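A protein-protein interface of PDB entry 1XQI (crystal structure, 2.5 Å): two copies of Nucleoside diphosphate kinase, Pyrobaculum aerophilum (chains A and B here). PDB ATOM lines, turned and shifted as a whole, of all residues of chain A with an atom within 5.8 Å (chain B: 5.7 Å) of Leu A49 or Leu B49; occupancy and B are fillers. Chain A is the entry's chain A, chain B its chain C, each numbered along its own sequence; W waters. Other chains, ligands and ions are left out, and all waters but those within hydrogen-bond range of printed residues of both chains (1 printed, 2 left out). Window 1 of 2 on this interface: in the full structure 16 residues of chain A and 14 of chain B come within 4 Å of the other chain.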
ATOM      1  N   VAL A  32       2.873 -11.479 -19.590  1.00  0.00           N
ATOM      2  CA  VAL A  32       1.601 -11.140 -19.040  1.00  0.00           C
ATOM      3  C   VAL A  32       0.558 -12.133 -19.517  1.00  0.00           C
ATOM      4  O   VAL A  32      -0.258 -12.545 -18.738  1.00  0.00           O
ATOM      5  CB  VAL A  32       1.208  -9.656 -19.324  1.00  0.00           C
ATOM      6  CG1 VAL A  32      -0.248  -9.412 -19.034  1.00  0.00           C
ATOM      7  CG2 VAL A  32       2.001  -8.775 -18.433  1.00  0.00           C
ATOM      8  N   ILE A  36      -1.599 -14.832 -17.188  1.00  0.00           N
ATOM      9  CA  ILE A  36      -3.029 -14.691 -17.192  1.00  0.00           C
ATOM     10  C   ILE A  36      -3.657 -16.001 -17.665  1.00  0.00           C
ATOM     11  O   ILE A  36      -4.625 -16.472 -17.055  1.00  0.00           O
ATOM     12  CB  ILE A  36      -3.466 -13.518 -18.044  1.00  0.00           C
ATOM     13  CG1 ILE A  36      -3.045 -12.227 -17.338  1.00  0.00           C
ATOM     14  CG2 ILE A  36      -5.013 -13.519 -18.255  1.00  0.00           C
ATOM     15  CD1 ILE A  36      -3.452 -10.974 -18.082  1.00  0.00           C
ATOM     16  N   ILE A  46     -10.317 -12.602 -13.336  1.00  0.00           N
ATOM     17  CA  ILE A  46      -9.638 -11.304 -13.098  1.00  0.00           C
ATOM     18  C   ILE A  46     -10.707 -10.228 -12.866  1.00  0.00           C
ATOM     19  O   ILE A  46     -11.517  -9.988 -13.735  1.00  0.00           O
ATOM     20  CB  ILE A  46      -8.787 -10.866 -14.311  1.00  0.00           C
ATOM     21  CG1 ILE A  46      -7.629 -11.846 -14.544  1.00  0.00           C
ATOM     22  CG2 ILE A  46      -8.318  -9.370 -14.181  1.00  0.00           C
ATOM     23  CD1 ILE A  46      -6.798 -11.512 -15.805  1.00  0.00           C
ATOM     24  N   VAL A  47     -10.722  -9.598 -11.692  1.00  0.00           N
ATOM     25  CA  VAL A  47     -11.749  -8.576 -11.379  1.00  0.00           C
ATOM     26  C   VAL A  47     -11.144  -7.145 -11.282  1.00  0.00           C
ATOM     27  O   VAL A  47     -11.869  -6.170 -11.050  1.00  0.00           O
ATOM     28  CB  VAL A  47     -12.578  -8.946 -10.077  1.00  0.00           C
ATOM     29  CG1 VAL A  47     -13.347 -10.292 -10.205  1.00  0.00           C
ATOM     30  CG2 VAL A  47     -11.721  -8.972  -8.876  1.00  0.00           C
ATOM     31  N   ALA A  48      -9.810  -7.040 -11.449  1.00  0.00           N
ATOM     32  CA  ALA A  48      -9.070  -5.777 -11.483  1.00  0.00           C
ATOM     33  C   ALA A  48      -7.731  -6.037 -12.171  1.00  0.00           C
ATOM     34  O   ALA A  48      -7.115  -7.089 -12.009  1.00  0.00           O
ATOM     35  CB  ALA A  48      -8.880  -5.192 -10.081  1.00  0.00           C
ATOM     36  N   LEU A  49      -7.309  -5.086 -12.985  1.00  0.00           N
ATOM     37  CA  LEU A  49      -6.136  -5.235 -13.819  1.00  0.00           C
ATOM     38  C   LEU A  49      -5.665  -3.859 -14.237  1.00  0.00           C
ATOM     39  O   LEU A  49      -6.444  -3.115 -14.793  1.00  0.00           O
ATOM     40  CB  LEU A  49      -6.488  -6.016 -15.075  1.00  0.00           C
ATOM     41  CG  LEU A  49      -5.461  -6.837 -15.891  1.00  0.00           C
ATOM     42  CD1 LEU A  49      -5.787  -6.638 -17.334  1.00  0.00           C
ATOM     43  CD2 LEU A  49      -4.093  -6.472 -15.671  1.00  0.00           C
ATOM     44  N   LYS A  50      -4.405  -3.515 -13.964  1.00  0.00           N
ATOM     45  CA  LYS A  50      -3.811  -2.325 -14.544  1.00  0.00           C
ATOM     46  C   LYS A  50      -2.302  -2.436 -14.682  1.00  0.00           C
ATOM     47  O   LYS A  50      -1.679  -3.119 -13.889  1.00  0.00           O
ATOM     48  CB  LYS A  50      -4.181  -1.079 -13.750  1.00  0.00           C
ATOM     49  CG  LYS A  50      -3.789  -1.061 -12.295  1.00  0.00           C
ATOM     50  CD  LYS A  50      -4.243   0.253 -11.726  1.00  0.00           C
ATOM     51  CE  LYS A  50      -3.956   0.345 -10.242  1.00  0.00           C
ATOM     52  NZ  LYS A  50      -4.811   1.429  -9.665  1.00  0.00           N
ATOM     53  N   MET A  51      -1.737  -1.799 -15.710  1.00  0.00           N
ATOM     54  CA  MET A  51      -0.278  -1.639 -15.849  1.00  0.00           C
ATOM     55  C   MET A  51       0.070  -0.310 -15.092  1.00  0.00           C
ATOM     56  O   MET A  51      -0.597   0.715 -15.286  1.00  0.00           O
ATOM     57  CB  MET A  51       0.151  -1.600 -17.330  1.00  0.00           C
ATOM     58  CG  MET A  51       1.648  -1.270 -17.511  1.00  0.00           C
ATOM     59  SD  MET A  51       2.198  -1.336 -19.243  1.00  0.00           S
ATOM     60  CE  MET A  51       2.089  -3.081 -19.426  1.00  0.00           C
ATOM     61  N   VAL A 118       2.302  -4.934 -13.570  1.00  0.00           N
ATOM     62  CA  VAL A 118       0.918  -5.169 -13.931  1.00  0.00           C
ATOM     63  C   VAL A 118       0.374  -5.792 -12.673  1.00  0.00           C
ATOM     64  O   VAL A 118       0.946  -6.767 -12.175  1.00  0.00           O
ATOM     65  CB  VAL A 118       0.800  -6.093 -15.193  1.00  0.00           C
ATOM     66  CG1 VAL A 118      -0.626  -6.688 -15.362  1.00  0.00           C
ATOM     67  CG2 VAL A 118       1.156  -5.298 -16.438  1.00  0.00           C
ATOM     68  N   VAL A 119      -0.675  -5.171 -12.132  1.00  0.00           N
ATOM     69  CA  VAL A 119      -1.339  -5.575 -10.907  1.00  0.00           C
ATOM     70  C   VAL A 119      -2.706  -6.172 -11.262  1.00  0.00           C
ATOM     71  O   VAL A 119      -3.451  -5.612 -12.086  1.00  0.00           O
ATOM     72  CB  VAL A 119      -1.568  -4.354  -9.972  1.00  0.00           C
ATOM     73  CG1 VAL A 119      -1.964  -4.826  -8.568  1.00  0.00           C
ATOM     74  CG2 VAL A 119      -0.280  -3.532  -9.855  1.00  0.00           C
ATOM     75  N   MET A 120      -3.052  -7.296 -10.650  1.00  0.00           N
ATOM     76  CA  MET A 120      -4.372  -7.896 -10.916  1.00  0.00           C
ATOM     77  C   MET A 120      -4.947  -8.424  -9.621  1.00  0.00           C
ATOM     78  O   MET A 120      -4.235  -8.734  -8.653  1.00  0.00           O
ATOM     79  CB  MET A 120      -4.339  -9.005 -12.052  1.00  0.00           C
ATOM     80  CG  MET A 120      -3.524 -10.270 -11.726  1.00  0.00           C
ATOM     81  SD  MET A 120      -3.368 -11.388 -13.144  1.00  0.00           S
ATOM     82  CE  MET A 120      -2.241 -10.338 -13.984  1.00  0.00           C
ATOM     83  N   VAL A 121      -6.269  -8.508  -9.606  1.00  0.00           N
ATOM     84  CA  VAL A 121      -6.959  -9.142  -8.484  1.00  0.00           C
ATOM     85  C   VAL A 121      -7.649 -10.356  -9.054  1.00  0.00           C
ATOM     86  O   VAL A 121      -8.301 -10.273 -10.104  1.00  0.00           O
ATOM     87  CB  VAL A 121      -7.932  -8.192  -7.824  1.00  0.00           C
ATOM     88  CG1 VAL A 121      -8.745  -8.903  -6.703  1.00  0.00           C
ATOM     89  CG2 VAL A 121      -7.164  -7.020  -7.226  1.00  0.00           C
ATOM     90  N   PHE A 188      -6.238  -0.403  -5.516  1.00  0.00           N
ATOM     91  CA  PHE A 188      -7.518  -0.184  -6.206  1.00  0.00           C
ATOM     92  C   PHE A 188      -8.549   0.565  -5.360  1.00  0.00           C
ATOM     93  O   PHE A 188      -8.782   0.213  -4.201  1.00  0.00           O
ATOM     94  CB  PHE A 188      -8.115  -1.522  -6.730  1.00  0.00           C
ATOM     95  CG  PHE A 188      -7.203  -2.257  -7.694  1.00  0.00           C
ATOM     96  CD1 PHE A 188      -6.401  -3.306  -7.252  1.00  0.00           C
ATOM     97  CD2 PHE A 188      -7.117  -1.870  -9.021  1.00  0.00           C
ATOM     98  CE1 PHE A 188      -5.546  -3.967  -8.096  1.00  0.00           C
ATOM     99  CE2 PHE A 188      -6.253  -2.529  -9.903  1.00  0.00           C
ATOM    100  CZ  PHE A 188      -5.464  -3.581  -9.443  1.00  0.00           C
ATOM    101  N   GLU A 192     -12.789   0.252  -8.955  1.00  0.00           N
ATOM    102  CA  GLU A 192     -11.949  -0.524  -9.868  1.00  0.00           C
ATOM    103  C   GLU A 192     -11.977  -2.030  -9.613  1.00  0.00           C
ATOM    104  O   GLU A 192     -11.605  -2.788 -10.502  1.00  0.00           O
ATOM    105  CB  GLU A 192     -10.503  -0.021  -9.848  1.00  0.00           C
ATOM    106  CG  GLU A 192     -10.316   1.414 -10.301  1.00  0.00           C
ATOM    107  CD  GLU A 192      -8.844   1.782 -10.444  1.00  0.00           C
ATOM    108  OE1 GLU A 192      -8.152   1.909  -9.399  1.00  0.00           O
ATOM    109  OE2 GLU A 192      -8.385   1.948 -11.607  1.00  0.00           O
ATOM    110  N   VAL B  32      -8.828 -12.076 -23.108  1.00  0.00           N
ATOM    111  CA  VAL B  32      -7.793 -11.107 -22.897  1.00  0.00           C
ATOM    112  C   VAL B  32      -6.410 -11.666 -23.205  1.00  0.00           C
ATOM    113  O   VAL B  32      -5.665 -11.047 -23.963  1.00  0.00           O
ATOM    114  CB  VAL B  32      -7.844 -10.453 -21.483  1.00  0.00           C
ATOM    115  CG1 VAL B  32      -6.732  -9.525 -21.344  1.00  0.00           C
ATOM    116  CG2 VAL B  32      -9.134  -9.646 -21.344  1.00  0.00           C
ATOM    117  N   ILE B  36      -3.957 -10.666 -26.218  1.00  0.00           N
ATOM    118  CA  ILE B  36      -2.676 -10.046 -25.937  1.00  0.00           C
ATOM    119  C   ILE B  36      -1.564 -10.825 -26.634  1.00  0.00           C
ATOM    120  O   ILE B  36      -0.608 -10.235 -27.152  1.00  0.00           O
ATOM    121  CB  ILE B  36      -2.397  -9.906 -24.425  1.00  0.00           C
ATOM    122  CG1 ILE B  36      -3.254  -8.785 -23.835  1.00  0.00           C
ATOM    123  CG2 ILE B  36      -0.889  -9.623 -24.135  1.00  0.00           C
ATOM    124  CD1 ILE B  36      -3.324  -8.815 -22.296  1.00  0.00           C
ATOM    125  N   ILE B  46       2.689  -3.574 -25.301  1.00  0.00           N
ATOM    126  CA  ILE B  46       1.606  -2.926 -24.547  1.00  0.00           C
ATOM    127  C   ILE B  46       2.238  -1.830 -23.676  1.00  0.00           C
ATOM    128  O   ILE B  46       3.014  -2.132 -22.795  1.00  0.00           O
ATOM    129  CB  ILE B  46       0.875  -3.891 -23.620  1.00  0.00           C
ATOM    130  CG1 ILE B  46       0.191  -4.996 -24.418  1.00  0.00           C
ATOM    131  CG2 ILE B  46      -0.139  -3.125 -22.736  1.00  0.00           C
ATOM    132  CD1 ILE B  46      -0.701  -5.845 -23.536  1.00  0.00           C
ATOM    133  N   VAL B  47       1.921  -0.562 -23.933  1.00  0.00           N
ATOM    134  CA  VAL B  47       2.464   0.510 -23.095  1.00  0.00           C
ATOM    135  C   VAL B  47       1.448   1.115 -22.105  1.00  0.00           C
ATOM    136  O   VAL B  47       1.818   1.961 -21.278  1.00  0.00           O
ATOM    137  CB  VAL B  47       3.219   1.581 -23.947  1.00  0.00           C
ATOM    138  CG1 VAL B  47       4.481   0.972 -24.546  1.00  0.00           C
ATOM    139  CG2 VAL B  47       2.336   2.193 -25.055  1.00  0.00           C
ATOM    140  N   ALA B  48       0.172   0.695 -22.171  1.00  0.00           N
ATOM    141  CA  ALA B  48      -0.824   0.999 -21.110  1.00  0.00           C
ATOM    142  C   ALA B  48      -1.887  -0.054 -21.098  1.00  0.00           C
ATOM    143  O   ALA B  48      -2.208  -0.640 -22.114  1.00  0.00           O
ATOM    144  CB  ALA B  48      -1.448   2.417 -21.270  1.00  0.00           C
ATOM    145  N   LEU B  49      -2.427  -0.337 -19.933  1.00  0.00           N
ATOM    146  CA  LEU B  49      -3.385  -1.438 -19.822  1.00  0.00           C
ATOM    147  C   LEU B  49      -4.237  -1.247 -18.594  1.00  0.00           C
ATOM    148  O   LEU B  49      -3.713  -0.949 -17.524  1.00  0.00           O
ATOM    149  CB  LEU B  49      -2.640  -2.779 -19.734  1.00  0.00           C
ATOM    150  CG  LEU B  49      -3.224  -4.180 -20.039  1.00  0.00           C
ATOM    151  CD1 LEU B  49      -2.782  -5.149 -18.938  1.00  0.00           C
ATOM    152  CD2 LEU B  49      -4.680  -4.231 -20.104  1.00  0.00           C
ATOM    153  N   LYS B  50      -5.551  -1.403 -18.732  1.00  0.00           N
ATOM    154  CA  LYS B  50      -6.421  -1.451 -17.538  1.00  0.00           C
ATOM    155  C   LYS B  50      -7.812  -2.031 -17.784  1.00  0.00           C
ATOM    156  O   LYS B  50      -8.376  -1.780 -18.835  1.00  0.00           O
ATOM    157  CB  LYS B  50      -6.520  -0.080 -16.850  1.00  0.00           C
ATOM    158  CG  LYS B  50      -7.211   0.977 -17.635  1.00  0.00           C
ATOM    159  CD  LYS B  50      -7.411   2.243 -16.775  1.00  0.00           C
ATOM    160  CE  LYS B  50      -7.923   3.425 -17.654  1.00  0.00           C
ATOM    161  NZ  LYS B  50      -7.245   4.679 -17.206  1.00  0.00           N
ATOM    162  N   MET B  51      -8.319  -2.827 -16.845  1.00  0.00           N
ATOM    163  CA  MET B  51      -9.740  -3.218 -16.805  1.00  0.00           C
ATOM    164  C   MET B  51     -10.579  -2.046 -16.160  1.00  0.00           C
ATOM    165  O   MET B  51     -10.206  -1.496 -15.115  1.00  0.00           O
ATOM    166  CB  MET B  51      -9.960  -4.525 -15.977  1.00  0.00           C
ATOM    167  CG  MET B  51     -11.299  -5.238 -16.209  1.00  0.00           C
ATOM    168  SD  MET B  51     -11.398  -6.763 -15.189  1.00  0.00           S
ATOM    169  CE  MET B  51     -11.167  -5.669 -13.896  1.00  0.00           C
ATOM    170  N   VAL B 118     -11.431  -4.002 -21.309  1.00  0.00           N
ATOM    171  CA  VAL B 118     -10.006  -3.867 -21.050  1.00  0.00           C
ATOM    172  C   VAL B 118      -9.483  -2.985 -22.159  1.00  0.00           C
ATOM    173  O   VAL B 118      -9.745  -3.282 -23.317  1.00  0.00           O
ATOM    174  CB  VAL B 118      -9.307  -5.246 -20.985  1.00  0.00           C
ATOM    175  CG1 VAL B 118      -7.785  -5.122 -21.075  1.00  0.00           C
ATOM    176  CG2 VAL B 118      -9.702  -5.988 -19.704  1.00  0.00           C
ATOM    177  N   VAL B 119      -8.813  -1.878 -21.796  1.00  0.00           N
ATOM    178  CA  VAL B 119      -8.276  -0.861 -22.696  1.00  0.00           C
ATOM    179  C   VAL B 119      -6.755  -0.981 -22.677  1.00  0.00           C
ATOM    180  O   VAL B 119      -6.134  -1.112 -21.608  1.00  0.00           O
ATOM    181  CB  VAL B 119      -8.646   0.602 -22.236  1.00  0.00           C
ATOM    182  CG1 VAL B 119      -8.438   1.601 -23.362  1.00  0.00           C
ATOM    183  CG2 VAL B 119     -10.121   0.725 -21.824  1.00  0.00           C
ATOM    184  N   MET B 120      -6.138  -0.940 -23.846  1.00  0.00           N
ATOM    185  CA  MET B 120      -4.688  -1.044 -23.919  1.00  0.00           C
ATOM    186  C   MET B 120      -4.179  -0.122 -25.027  1.00  0.00           C
ATOM    187  O   MET B 120      -4.878   0.215 -25.983  1.00  0.00           O
ATOM    188  CB  MET B 120      -4.174  -2.540 -24.067  1.00  0.00           C
ATOM    189  CG  MET B 120      -4.264  -3.155 -25.481  1.00  0.00           C
ATOM    190  SD  MET B 120      -4.081  -4.969 -25.536  1.00  0.00           S
ATOM    191  CE  MET B 120      -5.467  -5.434 -24.564  1.00  0.00           C
ATOM    192  N   VAL B 121      -2.940   0.304 -24.862  1.00  0.00           N
ATOM    193  CA  VAL B 121      -2.244   1.052 -25.897  1.00  0.00           C
ATOM    194  C   VAL B 121      -1.126   0.169 -26.437  1.00  0.00           C
ATOM    195  O   VAL B 121      -0.389  -0.436 -25.671  1.00  0.00           O
ATOM    196  CB  VAL B 121      -1.746   2.442 -25.381  1.00  0.00           C
ATOM    197  CG1 VAL B 121      -1.030   3.251 -26.516  1.00  0.00           C
ATOM    198  CG2 VAL B 121      -2.935   3.242 -24.855  1.00  0.00           C
ATOM    199  N   PHE B 188      -6.280   7.637 -20.843  1.00  0.00           N
ATOM    200  CA  PHE B 188      -5.044   7.608 -20.068  1.00  0.00           C
ATOM    201  C   PHE B 188      -4.443   8.985 -19.842  1.00  0.00           C
ATOM    202  O   PHE B 188      -4.277   9.745 -20.784  1.00  0.00           O
ATOM    203  CB  PHE B 188      -4.014   6.730 -20.774  1.00  0.00           C
ATOM    204  CG  PHE B 188      -4.422   5.306 -20.877  1.00  0.00           C
ATOM    205  CD1 PHE B 188      -4.900   4.790 -22.092  1.00  0.00           C
ATOM    206  CD2 PHE B 188      -4.342   4.472 -19.770  1.00  0.00           C
ATOM    207  CE1 PHE B 188      -5.286   3.463 -22.204  1.00  0.00           C
ATOM    208  CE2 PHE B 188      -4.742   3.130 -19.855  1.00  0.00           C
ATOM    209  CZ  PHE B 188      -5.219   2.617 -21.064  1.00  0.00           C
ATOM    210  N   GLU B 192       0.404   7.499 -17.485  1.00  0.00           N
ATOM    211  CA  GLU B 192      -0.105   6.133 -17.368  1.00  0.00           C
ATOM    212  C   GLU B 192       0.358   5.412 -18.636  1.00  0.00           C
ATOM    213  O   GLU B 192       0.282   4.176 -18.721  1.00  0.00           O
ATOM    214  CB  GLU B 192      -1.632   6.082 -17.298  1.00  0.00           C
ATOM    215  CG  GLU B 192      -2.324   6.515 -16.012  1.00  0.00           C
ATOM    216  CD  GLU B 192      -3.846   6.674 -16.223  1.00  0.00           C
ATOM    217  OE1 GLU B 192      -4.272   7.682 -16.824  1.00  0.00           O
ATOM    218  OE2 GLU B 192      -4.627   5.793 -15.812  1.00  0.00           O
HETATM  219  O   HOH W   1      -1.445   1.341 -17.878  1.00  0.00           O
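The backbone carbonyl oxygen (O) of Lys A50 sits at hydrogen-bond distance from the backbone NH (N) of Val A119, at 2.9 Å.
The side-chain amino group (NZ) of Lys A50 is in salt-bridge range of the side-chain carboxylate (OE1) of Glu A192, at 3.4 Å.
The backbone NH of Val A47 lies within hydrogen-bond range of the backbone carbonyl oxygen of Val A121 (3.0 Å).
The backbone carbonyl oxygen (O) of Val B121 lies within hydrogen-bond range of the backbone NH (N) of Val B47 (2.9 Å).
NZ of Lys B50 lies within salt-bridge range of OE2 of Glu B192, 3.2 Å away.
O of Ala A48 sits at hydrogen-bond distance from N of Val A121, 2.9 Å away.
Among the printed residues, merely in contact across the chains: Val A47 with Met B51, Ala A48 with Met B51, Leu A49 with Leu B49, Leu A49 with Lys B50, Lys A50 with Leu B49 and Met A51 with Val B47.
Water W1 lies within hydrogen-bond range of the backbone carbonyl oxygen of Met A51, the backbone NH of Leu B49 and the backbone carbonyl oxygen of Glu B192.
N of Met B51 sits at hydrogen-bond distance from O of Leu A49 (2.8 Å).
O of Ile A46 sits close to SD of Met B51, at 3.5 Å.
The side-chain sulfur (SD) of Met A51 lies close to the backbone carbonyl oxygen (O) of Ile B46, 3.7 Å away.
N of Met A51 lies within hydrogen-bond range of O of Leu B49, at 2.8 Å.
Ile A46 touches Met B51, and with the chains exchanged Met A51 touches Ile B46.
Ala A48 touches Met B51, but with the chains exchanged Met A51 does not touch Ala B48 (4.1 Å).
Leu A49 touches Lys B50, and with the chains exchanged Lys A50 touches Leu B49.
Leu A49 touches Met B51, and with the chains exchanged Met A51 touches Leu B49.
Of the 10 pairs that touch across the chains among the printed residues, 9 have their exchanged pair printed and touching as well.
Printed residues of chain B within 4 Å of Ile A46: Met B51 (3.5 Å).
Of the printed residues of chain B, Val A47 touches Met B51 (3.0 Å).
Of the printed residues of chain B, Ala A48 touches Met B51 (3.1 Å).
Leu A49 touches just these residues of chain B: Leu B49, Lys B50 and Met B51.
Of the printed residues of chain B, Met A51 touches Ile B46, Val B47 and Leu B49.
Of chain A, only Leu A49 (3.7 Å), Lys A50 (3.3 Å) and Met A51 (2.8 Å) come within 4 Å of Leu B49.
Of the printed residues of chain A, Lys B50 touches Leu A49.
Phe B188 touches none of the printed residues of chain A.
The nearest residue of chain B that does not touch Leu A49 is Val B118 (4.5 Å).
The nearest residue of chain A that does not touch Leu B49 is Val A118 (4.5 Å).
Of the 14 printed residues of chain A, 6 touch a printed residue of chain B.
Hydrophobic or aromatic side chains of chain A within 4 Å of the printed part of chain B: Leu A49 and Met A51.
Of the 14 printed residues of chain B, 5 touch a printed residue of chain A.
Hydrophobic or aromatic side chains of chain B within 4 Å of the printed part of chain A: Ile B46, Leu B49 and Met B51.
Along chain B the printed residues that touch a printed residue of chain A span positions 46 to 51.
Among the printed residues, no Asp or Glu carboxylate lies within 4 Å of a Lys or Arg side-chain nitrogen of the other chain.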
